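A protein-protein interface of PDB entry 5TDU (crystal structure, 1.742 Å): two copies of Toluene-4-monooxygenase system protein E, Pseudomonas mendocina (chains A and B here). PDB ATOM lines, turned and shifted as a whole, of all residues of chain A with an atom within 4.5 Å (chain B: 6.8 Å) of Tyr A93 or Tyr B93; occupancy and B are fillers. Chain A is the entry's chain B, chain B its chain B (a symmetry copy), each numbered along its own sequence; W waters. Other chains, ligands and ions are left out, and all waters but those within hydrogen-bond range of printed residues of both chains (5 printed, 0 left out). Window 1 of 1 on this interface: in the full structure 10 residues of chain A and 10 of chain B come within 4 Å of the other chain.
O of Ser A92 sits at hydrogen-bond distance from OG of Ser A96 (3.0 Å). The backbone carbonyl oxygen of Ser B92 sits at hydrogen-bond distance from the side-chain hydroxyl of Ser B96.
Tyr B93 touches its own counterpart, Tyr A93. Tyr A93 touches Ser B96, and with the chains exchanged Ser A96 touches Tyr B93. Tyr A93 touches Leu B97, and with the chains exchanged Leu A97 touches Tyr B93. Tyr A93 touches Gln B100, and with the chains exchanged Gln A100 touches Tyr B93. Positions printed for both chains: 89, 90, 91, 92, 93, 94, 95, 96, 97, 100 and 249.
Among the printed residues, pairs that only touch across the chains: Ser A96 with Tyr B93, Tyr A93 with Ser B96, Tyr A93 with Tyr B93, Tyr A93 with Leu B97, Leu A97 with Tyr B93, Gln A100 with Tyr B93, Tyr A93 with Gln B100 and Leu A249 with Phe B101.
Water W4 bridges the side-chain amide nitrogen (NE2) of Gln B90 (2.8 Å) and the side-chain hydroxyl (OG) of Ser A96 (3.2 Å). Water W2 bridges the side-chain amide nitrogen of Gln A90 and the side-chain hydroxyl of Ser B96. Water W3 lies within hydrogen-bond range of NE2 of Gln A90 and OG of Ser B96. Water W5 bridges NE2 of Gln B90 (2.8 Å) and OG of Ser A96 (3.0 Å). Water W1 bridges the backbone carbonyl oxygen (O) of Ser A96 (2.9 Å) and the side-chain amino group (NZ) of Lys B256 (3.4 Å).
Printed residues of chain B within 4 Å of Tyr A93: Tyr B93, Ser B96, Leu B97 and Gln B100. Printed residues of chain B within 4 Å of Gln A100: Tyr B93 (3.97 Å) and Asp B252 (2.8 Å). Of the printed residues of chain B, Leu A249 touches Phe B101 (3.98 Å). Of the printed residues of chain A, Tyr B93 touches Tyr A93, Ser A96, Leu A97 and Gln A100. Printed residues of chain A within 4 Å of Leu B97: Tyr A93. Lys B256 touches none of the printed residues of chain A. The nearest printed residue of chain B that does not touch Leu A97 is Leu B97 (4.1 Å).
OD2 of Asp B252 lies close to OE1 of Gln A100 (2.8 Å).
Of the 20 printed residues of chain B, 6 touch a printed residue of chain A. Among the printed residues, no Asp or Glu carboxylate lies within 4 Å of a Lys or Arg side-chain nitrogen of the other chain.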
ATOM      1  N   GLY A  89      23.417   5.138 -20.115  1.00  0.00           N
ATOM      2  CA  GLY A  89      23.626   5.853 -21.364  1.00  0.00           C
ATOM      3  C   GLY A  89      22.352   6.488 -21.901  1.00  0.00           C
ATOM      4  O   GLY A  89      22.310   7.692 -22.163  1.00  0.00           O
ATOM      5  N   GLN A  90      21.306   5.686 -22.063  1.00  0.00           N
ATOM      6  CA  GLN A  90      20.048   6.191 -22.620  1.00  0.00           C
ATOM      7  C   GLN A  90      19.362   7.163 -21.670  1.00  0.00           C
ATOM      8  O   GLN A  90      18.769   8.147 -22.100  1.00  0.00           O
ATOM      9  CB  GLN A  90      19.086   5.037 -22.950  1.00  0.00           C
ATOM     10  CG  GLN A  90      19.229   4.486 -24.360  1.00  0.00           C
ATOM     11  CD  GLN A  90      18.986   5.548 -25.430  1.00  0.00           C
ATOM     12  OE1 GLN A  90      17.859   6.030 -25.618  1.00  0.00           O
ATOM     13  NE2 GLN A  90      20.048   5.934 -26.117  1.00  0.00           N
ATOM     14  N   GLU A  91      19.413   6.884 -20.375  1.00  0.00           N
ATOM     15  CA  GLU A  91      18.721   7.751 -19.422  1.00  0.00           C
ATOM     16  C   GLU A  91      19.493   9.064 -19.206  1.00  0.00           C
ATOM     17  O   GLU A  91      18.884  10.126 -19.066  1.00  0.00           O
ATOM     18  CB  GLU A  91      18.490   7.020 -18.104  1.00  0.00           C
ATOM     19  CG  GLU A  91      17.546   7.737 -17.145  1.00  0.00           C
ATOM     20  CD  GLU A  91      16.147   7.994 -17.720  1.00  0.00           C
ATOM     21  OE1 GLU A  91      15.804   7.436 -18.782  1.00  0.00           O
ATOM     22  OE2 GLU A  91      15.380   8.756 -17.091  1.00  0.00           O
ATOM     23  N   SER A  92      20.823   9.022 -19.207  1.00  0.00           N
ATOM     24  CA  SER A  92      21.580  10.264 -19.104  1.00  0.00           C
ATOM     25  C   SER A  92      21.285  11.146 -20.315  1.00  0.00           C
ATOM     26  O   SER A  92      21.179  12.366 -20.190  1.00  0.00           O
ATOM     27  CB  SER A  92      23.077   9.985 -18.985  1.00  0.00           C
ATOM     28  OG  SER A  92      23.358   9.396 -17.731  1.00  0.00           O
ATOM     29  N   TYR A  93      21.136  10.523 -21.480  1.00  0.00           N
ATOM     30  CA  TYR A  93      20.752  11.230 -22.700  1.00  0.00           C
ATOM     31  C   TYR A  93      19.372  11.888 -22.538  1.00  0.00           C
ATOM     32  O   TYR A  93      19.216  13.075 -22.815  1.00  0.00           O
ATOM     33  CB  TYR A  93      20.786  10.256 -23.883  1.00  0.00           C
ATOM     34  CG  TYR A  93      19.990  10.653 -25.104  1.00  0.00           C
ATOM     35  CD1 TYR A  93      20.416  11.674 -25.952  1.00  0.00           C
ATOM     36  CD2 TYR A  93      18.818   9.976 -25.438  1.00  0.00           C
ATOM     37  CE1 TYR A  93      19.673  12.020 -27.097  1.00  0.00           C
ATOM     38  CE2 TYR A  93      18.082  10.315 -26.563  1.00  0.00           C
ATOM     39  CZ  TYR A  93      18.510  11.332 -27.388  1.00  0.00           C
ATOM     40  OH  TYR A  93      17.754  11.646 -28.503  1.00  0.00           O
ATOM     41  N   VAL A  94      18.384  11.142 -22.045  1.00  0.00           N
ATOM     42  CA  VAL A  94      17.038  11.701 -21.873  1.00  0.00           C
ATOM     43  C   VAL A  94      17.049  12.823 -20.846  1.00  0.00           C
ATOM     44  O   VAL A  94      16.399  13.851 -21.041  1.00  0.00           O
ATOM     45  CB  VAL A  94      16.009  10.622 -21.464  1.00  0.00           C
ATOM     46  CG1 VAL A  94      14.737  11.285 -20.949  1.00  0.00           C
ATOM     47  CG2 VAL A  94      15.691   9.712 -22.649  1.00  0.00           C
ATOM     48  N   GLN A  95      17.770  12.628 -19.744  1.00  0.00           N
ATOM     49  CA  GLN A  95      17.858  13.670 -18.719  1.00  0.00           C
ATOM     50  C   GLN A  95      18.535  14.929 -19.276  1.00  0.00           C
ATOM     51  O   GLN A  95      18.167  16.049 -18.915  1.00  0.00           O
ATOM     52  CB  GLN A  95      18.604  13.155 -17.476  1.00  0.00           C
ATOM     53  CG  GLN A  95      17.888  11.991 -16.748  1.00  0.00           C
ATOM     54  CD  GLN A  95      16.517  12.375 -16.173  1.00  0.00           C
ATOM     55  OE1 GLN A  95      16.391  13.373 -15.472  1.00  0.00           O
ATOM     56  NE2 GLN A  95      15.487  11.569 -16.469  1.00  0.00           N
ATOM     57  N   SER A  96      19.520  14.748 -20.152  1.00  0.00           N
ATOM     58  CA  SER A  96      20.161  15.885 -20.824  1.00  0.00           C
ATOM     59  C   SER A  96      19.203  16.587 -21.784  1.00  0.00           C
ATOM     60  O   SER A  96      19.247  17.832 -21.930  1.00  0.00           O
ATOM     61  CB  SER A  96      21.424  15.433 -21.578  1.00  0.00           C
ATOM     62  OG  SER A  96      22.454  15.077 -20.666  1.00  0.00           O
ATOM     63  N   LEU A  97      18.351  15.808 -22.449  1.00  0.00           N
ATOM     64  CA  LEU A  97      17.288  16.408 -23.270  1.00  0.00           C
ATOM     65  C   LEU A  97      16.351  17.268 -22.412  1.00  0.00           C
ATOM     66  O   LEU A  97      16.004  18.399 -22.790  1.00  0.00           O
ATOM     67  CB  LEU A  97      16.474  15.341 -24.000  1.00  0.00           C
ATOM     68  CG  LEU A  97      17.089  14.633 -25.200  1.00  0.00           C
ATOM     69  CD1 LEU A  97      16.184  13.471 -25.597  1.00  0.00           C
ATOM     70  CD2 LEU A  97      17.295  15.599 -26.378  1.00  0.00           C
ATOM     71  N   GLN A 100      18.230  20.552 -21.386  1.00  0.00           N
ATOM     72  CA  GLN A 100      18.426  21.483 -22.490  1.00  0.00           C
ATOM     73  C   GLN A 100      17.112  22.047 -23.022  1.00  0.00           C
ATOM     74  O   GLN A 100      17.025  23.237 -23.324  1.00  0.00           O
ATOM     75  CB  GLN A 100      19.203  20.809 -23.626  1.00  0.00           C
ATOM     76  CG  GLN A 100      19.488  21.747 -24.796  1.00  0.00           C
ATOM     77  CD  GLN A 100      20.173  23.031 -24.356  1.00  0.00           C
ATOM     78  OE1 GLN A 100      19.826  24.124 -24.809  1.00  0.00           O
ATOM     79  NE2 GLN A 100      21.140  22.907 -23.459  1.00  0.00           N
ATOM     80  N   LEU A 249      11.297  12.793 -29.239  1.00  0.00           N
ATOM     81  CA  LEU A 249      12.615  12.278 -28.847  1.00  0.00           C
ATOM     82  C   LEU A 249      12.522  11.373 -27.612  1.00  0.00           C
ATOM     83  O   LEU A 249      13.181  10.342 -27.540  1.00  0.00           O
ATOM     84  CB  LEU A 249      13.597  13.427 -28.577  1.00  0.00           C
ATOM     85  CG  LEU A 249      14.020  14.209 -29.827  1.00  0.00           C
ATOM     86  CD1 LEU A 249      14.730  15.506 -29.452  1.00  0.00           C
ATOM     87  CD2 LEU A 249      14.907  13.351 -30.734  1.00  0.00           C
ATOM     88  N   GLN B  87      32.518  15.479 -19.377  1.00  0.00           N
ATOM     89  CA  GLN B  87      32.492  15.482 -20.836  1.00  0.00           C
ATOM     90  C   GLN B  87      32.049  14.135 -21.409  1.00  0.00           C
ATOM     91  O   GLN B  87      31.503  14.090 -22.496  1.00  0.00           O
ATOM     92  CB  GLN B  87      33.851  15.895 -21.393  1.00  0.00           C
ATOM     93  CG  GLN B  87      34.192  17.360 -21.059  1.00  0.00           C
ATOM     94  CD  GLN B  87      33.171  18.350 -21.616  1.00  0.00           C
ATOM     95  OE1 GLN B  87      32.093  18.544 -21.046  1.00  0.00           O
ATOM     96  NE2 GLN B  87      33.523  19.005 -22.716  1.00  0.00           N
ATOM     97  N   ASP B  88      32.237  13.042 -20.679  1.00  0.00           N
ATOM     98  CA  ASP B  88      31.668  11.781 -21.158  1.00  0.00           C
ATOM     99  C   ASP B  88      30.146  11.916 -21.136  1.00  0.00           C
ATOM    100  O   ASP B  88      29.446  11.422 -22.026  1.00  0.00           O
ATOM    101  CB  ASP B  88      32.131  10.598 -20.314  1.00  0.00           C
ATOM    102  CG  ASP B  88      31.718   9.259 -20.903  1.00  0.00           C
ATOM    103  OD1 ASP B  88      31.769   9.086 -22.141  1.00  0.00           O
ATOM    104  OD2 ASP B  88      31.351   8.366 -20.119  1.00  0.00           O
ATOM    105  N   GLY B  89      29.633  12.619 -20.131  1.00  0.00           N
ATOM    106  CA  GLY B  89      28.210  12.911 -20.084  1.00  0.00           C
ATOM    107  C   GLY B  89      27.734  13.725 -21.278  1.00  0.00           C
ATOM    108  O   GLY B  89      26.802  13.330 -21.981  1.00  0.00           O
ATOM    109  N   GLN B  90      28.374  14.865 -21.518  1.00  0.00           N
ATOM    110  CA  GLN B  90      27.961  15.745 -22.614  1.00  0.00           C
ATOM    111  C   GLN B  90      28.233  15.116 -23.974  1.00  0.00           C
ATOM    112  O   GLN B  90      27.450  15.272 -24.905  1.00  0.00           O
ATOM    113  CB  GLN B  90      28.674  17.105 -22.531  1.00  0.00           C
ATOM    114  CG  GLN B  90      27.934  18.151 -21.712  1.00  0.00           C
ATOM    115  CD  GLN B  90      26.541  18.445 -22.262  1.00  0.00           C
ATOM    116  OE1 GLN B  90      26.383  19.028 -23.345  1.00  0.00           O
ATOM    117  NE2 GLN B  90      25.525  18.021 -21.528  1.00  0.00           N
ATOM    118  N   GLU B  91      29.355  14.422 -24.108  1.00  0.00           N
ATOM    119  CA  GLU B  91      29.696  13.846 -25.409  1.00  0.00           C
ATOM    120  C   GLU B  91      28.847  12.597 -25.701  1.00  0.00           C
ATOM    121  O   GLU B  91      28.443  12.375 -26.844  1.00  0.00           O
ATOM    122  CB  GLU B  91      31.188  13.533 -25.480  1.00  0.00           C
ATOM    123  CG  GLU B  91      31.689  13.182 -26.877  1.00  0.00           C
ATOM    124  CD  GLU B  91      31.452  14.282 -27.920  1.00  0.00           C
ATOM    125  OE1 GLU B  91      31.096  15.419 -27.549  1.00  0.00           O
ATOM    126  OE2 GLU B  91      31.637  14.002 -29.126  1.00  0.00           O
ATOM    127  N   SER B  92      28.541  11.790 -24.687  1.00  0.00           N
ATOM    128  CA  SER B  92      27.655  10.655 -24.917  1.00  0.00           C
ATOM    129  C   SER B  92      26.282  11.156 -25.357  1.00  0.00           C
ATOM    130  O   SER B  92      25.643  10.554 -26.219  1.00  0.00           O
ATOM    131  CB  SER B  92      27.543   9.786 -23.666  1.00  0.00           C
ATOM    132  OG  SER B  92      28.770   9.126 -23.427  1.00  0.00           O
ATOM    133  N   TYR B  93      25.842  12.267 -24.775  1.00  0.00           N
ATOM    134  CA  TYR B  93      24.593  12.914 -25.171  1.00  0.00           C
ATOM    135  C   TYR B  93      24.649  13.354 -26.643  1.00  0.00           C
ATOM    136  O   TYR B  93      23.744  13.046 -27.416  1.00  0.00           O
ATOM    137  CB  TYR B  93      24.311  14.093 -24.232  1.00  0.00           C
ATOM    138  CG  TYR B  93      23.358  15.146 -24.744  1.00  0.00           C
ATOM    139  CD1 TYR B  93      21.987  14.908 -24.830  1.00  0.00           C
ATOM    140  CD2 TYR B  93      23.824  16.408 -25.108  1.00  0.00           C
ATOM    141  CE1 TYR B  93      21.108  15.907 -25.290  1.00  0.00           C
ATOM    142  CE2 TYR B  93      22.961  17.395 -25.564  1.00  0.00           C
ATOM    143  CZ  TYR B  93      21.610  17.143 -25.653  1.00  0.00           C
ATOM    144  OH  TYR B  93      20.775  18.146 -26.111  1.00  0.00           O
ATOM    145  N   VAL B  94      25.725  14.026 -27.048  1.00  0.00           N
ATOM    146  CA  VAL B  94      25.842  14.487 -28.437  1.00  0.00           C
ATOM    147  C   VAL B  94      25.904  13.303 -29.392  1.00  0.00           C
ATOM    148  O   VAL B  94      25.282  13.329 -30.455  1.00  0.00           O
ATOM    149  CB  VAL B  94      27.074  15.397 -28.645  1.00  0.00           C
ATOM    150  CG1 VAL B  94      27.361  15.550 -30.135  1.00  0.00           C
ATOM    151  CG2 VAL B  94      26.839  16.765 -28.007  1.00  0.00           C
ATOM    152  N   GLN B  95      26.663  12.273 -29.029  1.00  0.00           N
ATOM    153  CA  GLN B  95      26.753  11.082 -29.878  1.00  0.00           C
ATOM    154  C   GLN B  95      25.388  10.394 -30.002  1.00  0.00           C
ATOM    155  O   GLN B  95      25.051   9.857 -31.059  1.00  0.00           O
ATOM    156  CB  GLN B  95      27.810  10.102 -29.337  1.00  0.00           C
ATOM    157  CG  GLN B  95      29.253  10.664 -29.346  1.00  0.00           C
ATOM    158  CD  GLN B  95      29.784  10.977 -30.752  1.00  0.00           C
ATOM    159  OE1 GLN B  95      29.715  10.140 -31.646  1.00  0.00           O
ATOM    160  NE2 GLN B  95      30.322  12.190 -30.942  1.00  0.00           N
ATOM    161  N   SER B  96      24.604  10.408 -28.927  1.00  0.00           N
ATOM    162  CA  SER B  96      23.239   9.871 -28.971  1.00  0.00           C
ATOM    163  C   SER B  96      22.329  10.717 -29.860  1.00  0.00           C
ATOM    164  O   SER B  96      21.435  10.176 -30.554  1.00  0.00           O
ATOM    165  CB  SER B  96      22.645   9.769 -27.556  1.00  0.00           C
ATOM    166  OG  SER B  96      23.285   8.740 -26.814  1.00  0.00           O
ATOM    167  N   LEU B  97      22.532  12.034 -29.837  1.00  0.00           N
ATOM    168  CA  LEU B  97      21.815  12.909 -30.777  1.00  0.00           C
ATOM    169  C   LEU B  97      22.152  12.547 -32.229  1.00  0.00           C
ATOM    170  O   LEU B  97      21.255  12.448 -33.082  1.00  0.00           O
ATOM    171  CB  LEU B  97      22.140  14.382 -30.530  1.00  0.00           C
ATOM    172  CG  LEU B  97      21.536  15.081 -29.319  1.00  0.00           C
ATOM    173  CD1 LEU B  97      22.190  16.451 -29.171  1.00  0.00           C
ATOM    174  CD2 LEU B  97      20.010  15.209 -29.448  1.00  0.00           C
ATOM    175  N   PHE B  98      23.441  12.350 -32.507  1.00  0.00           N
ATOM    176  CA  PHE B  98      23.882  11.961 -33.856  1.00  0.00           C
ATOM    177  C   PHE B  98      23.193  10.663 -34.283  1.00  0.00           C
ATOM    178  O   PHE B  98      22.669  10.551 -35.389  1.00  0.00           O
ATOM    179  CB  PHE B  98      25.403  11.769 -33.917  1.00  0.00           C
ATOM    180  CG  PHE B  98      26.202  13.046 -33.838  1.00  0.00           C
ATOM    181  CD1 PHE B  98      27.583  12.985 -33.681  1.00  0.00           C
ATOM    182  CD2 PHE B  98      25.591  14.295 -33.936  1.00  0.00           C
ATOM    183  CE1 PHE B  98      28.356  14.152 -33.617  1.00  0.00           C
ATOM    184  CE2 PHE B  98      26.350  15.463 -33.866  1.00  0.00           C
ATOM    185  CZ  PHE B  98      27.737  15.391 -33.712  1.00  0.00           C
ATOM    186  N   GLN B 100      20.402   9.156 -33.127  1.00  0.00           N
ATOM    187  CA  GLN B 100      18.955   9.262 -33.261  1.00  0.00           C
ATOM    188  C   GLN B 100      18.537  10.134 -34.442  1.00  0.00           C
ATOM    189  O   GLN B 100      17.595   9.796 -35.159  1.00  0.00           O
ATOM    190  CB  GLN B 100      18.336   9.805 -31.969  1.00  0.00           C
ATOM    191  CG  GLN B 100      16.814   9.892 -32.023  1.00  0.00           C
ATOM    192  CD  GLN B 100      16.171   8.574 -32.422  1.00  0.00           C
ATOM    193  OE1 GLN B 100      15.241   8.539 -33.231  1.00  0.00           O
ATOM    194  NE2 GLN B 100      16.672   7.480 -31.866  1.00  0.00           N
ATOM    195  N   PHE B 101      19.233  11.246 -34.665  1.00  0.00           N
ATOM    196  CA  PHE B 101      18.859  12.107 -35.780  1.00  0.00           C
ATOM    197  C   PHE B 101      19.198  11.429 -37.107  1.00  0.00           C
ATOM    198  O   PHE B 101      18.506  11.617 -38.103  1.00  0.00           O
ATOM    199  CB  PHE B 101      19.527  13.482 -35.656  1.00  0.00           C
ATOM    200  CG  PHE B 101      18.765  14.436 -34.777  1.00  0.00           C
ATOM    201  CD1 PHE B 101      18.085  15.519 -35.324  1.00  0.00           C
ATOM    202  CD2 PHE B 101      18.691  14.224 -33.412  1.00  0.00           C
ATOM    203  CE1 PHE B 101      17.363  16.392 -34.511  1.00  0.00           C
ATOM    204  CE2 PHE B 101      17.970  15.087 -32.594  1.00  0.00           C
ATOM    205  CZ  PHE B 101      17.308  16.172 -33.141  1.00  0.00           C
ATOM    206  N   ARG B 161      37.480  18.619 -29.399  1.00  0.00           N
ATOM    207  CA  ARG B 161      36.127  18.085 -29.355  1.00  0.00           C
ATOM    208  C   ARG B 161      35.283  18.741 -30.458  1.00  0.00           C
ATOM    209  O   ARG B 161      34.602  18.051 -31.226  1.00  0.00           O
ATOM    210  CB  ARG B 161      35.495  18.323 -27.979  1.00  0.00           C
ATOM    211  CG  ARG B 161      34.006  17.944 -27.908  1.00  0.00           C
ATOM    212  CD  ARG B 161      33.363  18.336 -26.561  1.00  0.00           C
ATOM    213  NE  ARG B 161      32.035  17.732 -26.469  1.00  0.00           N
ATOM    214  CZ  ARG B 161      30.907  18.375 -26.195  1.00  0.00           C
ATOM    215  NH1 ARG B 161      29.766  17.692 -26.182  1.00  0.00           N
ATOM    216  NH2 ARG B 161      30.908  19.686 -25.934  1.00  0.00           N
ATOM    217  N   LEU B 249      21.129  22.059 -31.414  1.00  0.00           N
ATOM    218  CA  LEU B 249      21.411  21.247 -30.224  1.00  0.00           C
ATOM    219  C   LEU B 249      22.913  20.984 -30.063  1.00  0.00           C
ATOM    220  O   LEU B 249      23.444  21.029 -28.959  1.00  0.00           O
ATOM    221  CB  LEU B 249      20.652  19.914 -30.273  1.00  0.00           C
ATOM    222  CG  LEU B 249      19.132  20.041 -30.108  1.00  0.00           C
ATOM    223  CD1 LEU B 249      18.427  18.740 -30.479  1.00  0.00           C
ATOM    224  CD2 LEU B 249      18.771  20.463 -28.681  1.00  0.00           C
ATOM    225  N   LEU B 250      23.589  20.692 -31.170  1.00  0.00           N
ATOM    226  CA  LEU B 250      25.032  20.485 -31.139  1.00  0.00           C
ATOM    227  C   LEU B 250      25.737  21.743 -30.641  1.00  0.00           C
ATOM    228  O   LEU B 250      26.606  21.684 -29.766  1.00  0.00           O
ATOM    229  CB  LEU B 250      25.552  20.099 -32.524  1.00  0.00           C
ATOM    230  CG  LEU B 250      27.075  19.980 -32.656  1.00  0.00           C
ATOM    231  CD1 LEU B 250      27.608  18.937 -31.683  1.00  0.00           C
ATOM    232  CD2 LEU B 250      27.463  19.641 -34.090  1.00  0.00           C
ATOM    233  N   ASP B 252      24.527  24.141 -28.869  1.00  0.00           N
ATOM    234  CA  ASP B 252      24.241  24.396 -27.462  1.00  0.00           C
ATOM    235  C   ASP B 252      25.240  23.646 -26.574  1.00  0.00           C
ATOM    236  O   ASP B 252      25.702  24.189 -25.573  1.00  0.00           O
ATOM    237  CB  ASP B 252      22.801  24.014 -27.099  1.00  0.00           C
ATOM    238  CG  ASP B 252      21.820  25.141 -27.342  1.00  0.00           C
ATOM    239  OD1 ASP B 252      22.263  26.294 -27.514  1.00  0.00           O
ATOM    240  OD2 ASP B 252      20.601  24.881 -27.344  1.00  0.00           O
ATOM    241  N   SER B 253      25.587  22.412 -26.940  1.00  0.00           N
ATOM    242  CA  SER B 253      26.580  21.653 -26.183  1.00  0.00           C
ATOM    243  C   SER B 253      27.967  22.301 -26.298  1.00  0.00           C
ATOM    244  O   SER B 253      28.709  22.403 -25.321  1.00  0.00           O
ATOM    245  CB  SER B 253      26.626  20.192 -26.659  1.00  0.00           C
ATOM    246  OG  SER B 253      27.530  19.418 -25.875  1.00  0.00           O
ATOM    247  N   LYS B 256      28.282  25.337 -24.075  1.00  0.00           N
ATOM    248  CA  LYS B 256      28.575  25.043 -22.673  1.00  0.00           C
ATOM    249  C   LYS B 256      30.084  25.067 -22.435  1.00  0.00           C
ATOM    250  O   LYS B 256      30.558  25.623 -21.441  1.00  0.00           O
ATOM    251  CB  LYS B 256      27.994  23.688 -22.246  1.00  0.00           C
ATOM    252  CG  LYS B 256      26.493  23.686 -22.086  1.00  0.00           C
ATOM    253  CD  LYS B 256      26.002  22.360 -21.508  1.00  0.00           C
ATOM    254  CE  LYS B 256      24.531  22.458 -21.089  1.00  0.00           C
ATOM    255  NZ  LYS B 256      24.053  21.201 -20.449  1.00  0.00           N
HETATM  256  O   HOH W   1      21.866  18.956 -21.834  1.00  0.00           O
HETATM  257  O   HOH W   2      22.786   5.785 -25.605  1.00  0.00           O
HETATM  258  O   HOH W   3      22.006   6.401 -28.133  1.00  0.00           O
HETATM  259  O   HOH W   4      25.314  16.076 -19.540  1.00  0.00           O
HETATM  260  O   HOH W   5      23.250  17.817 -19.826  1.00  0.00           O
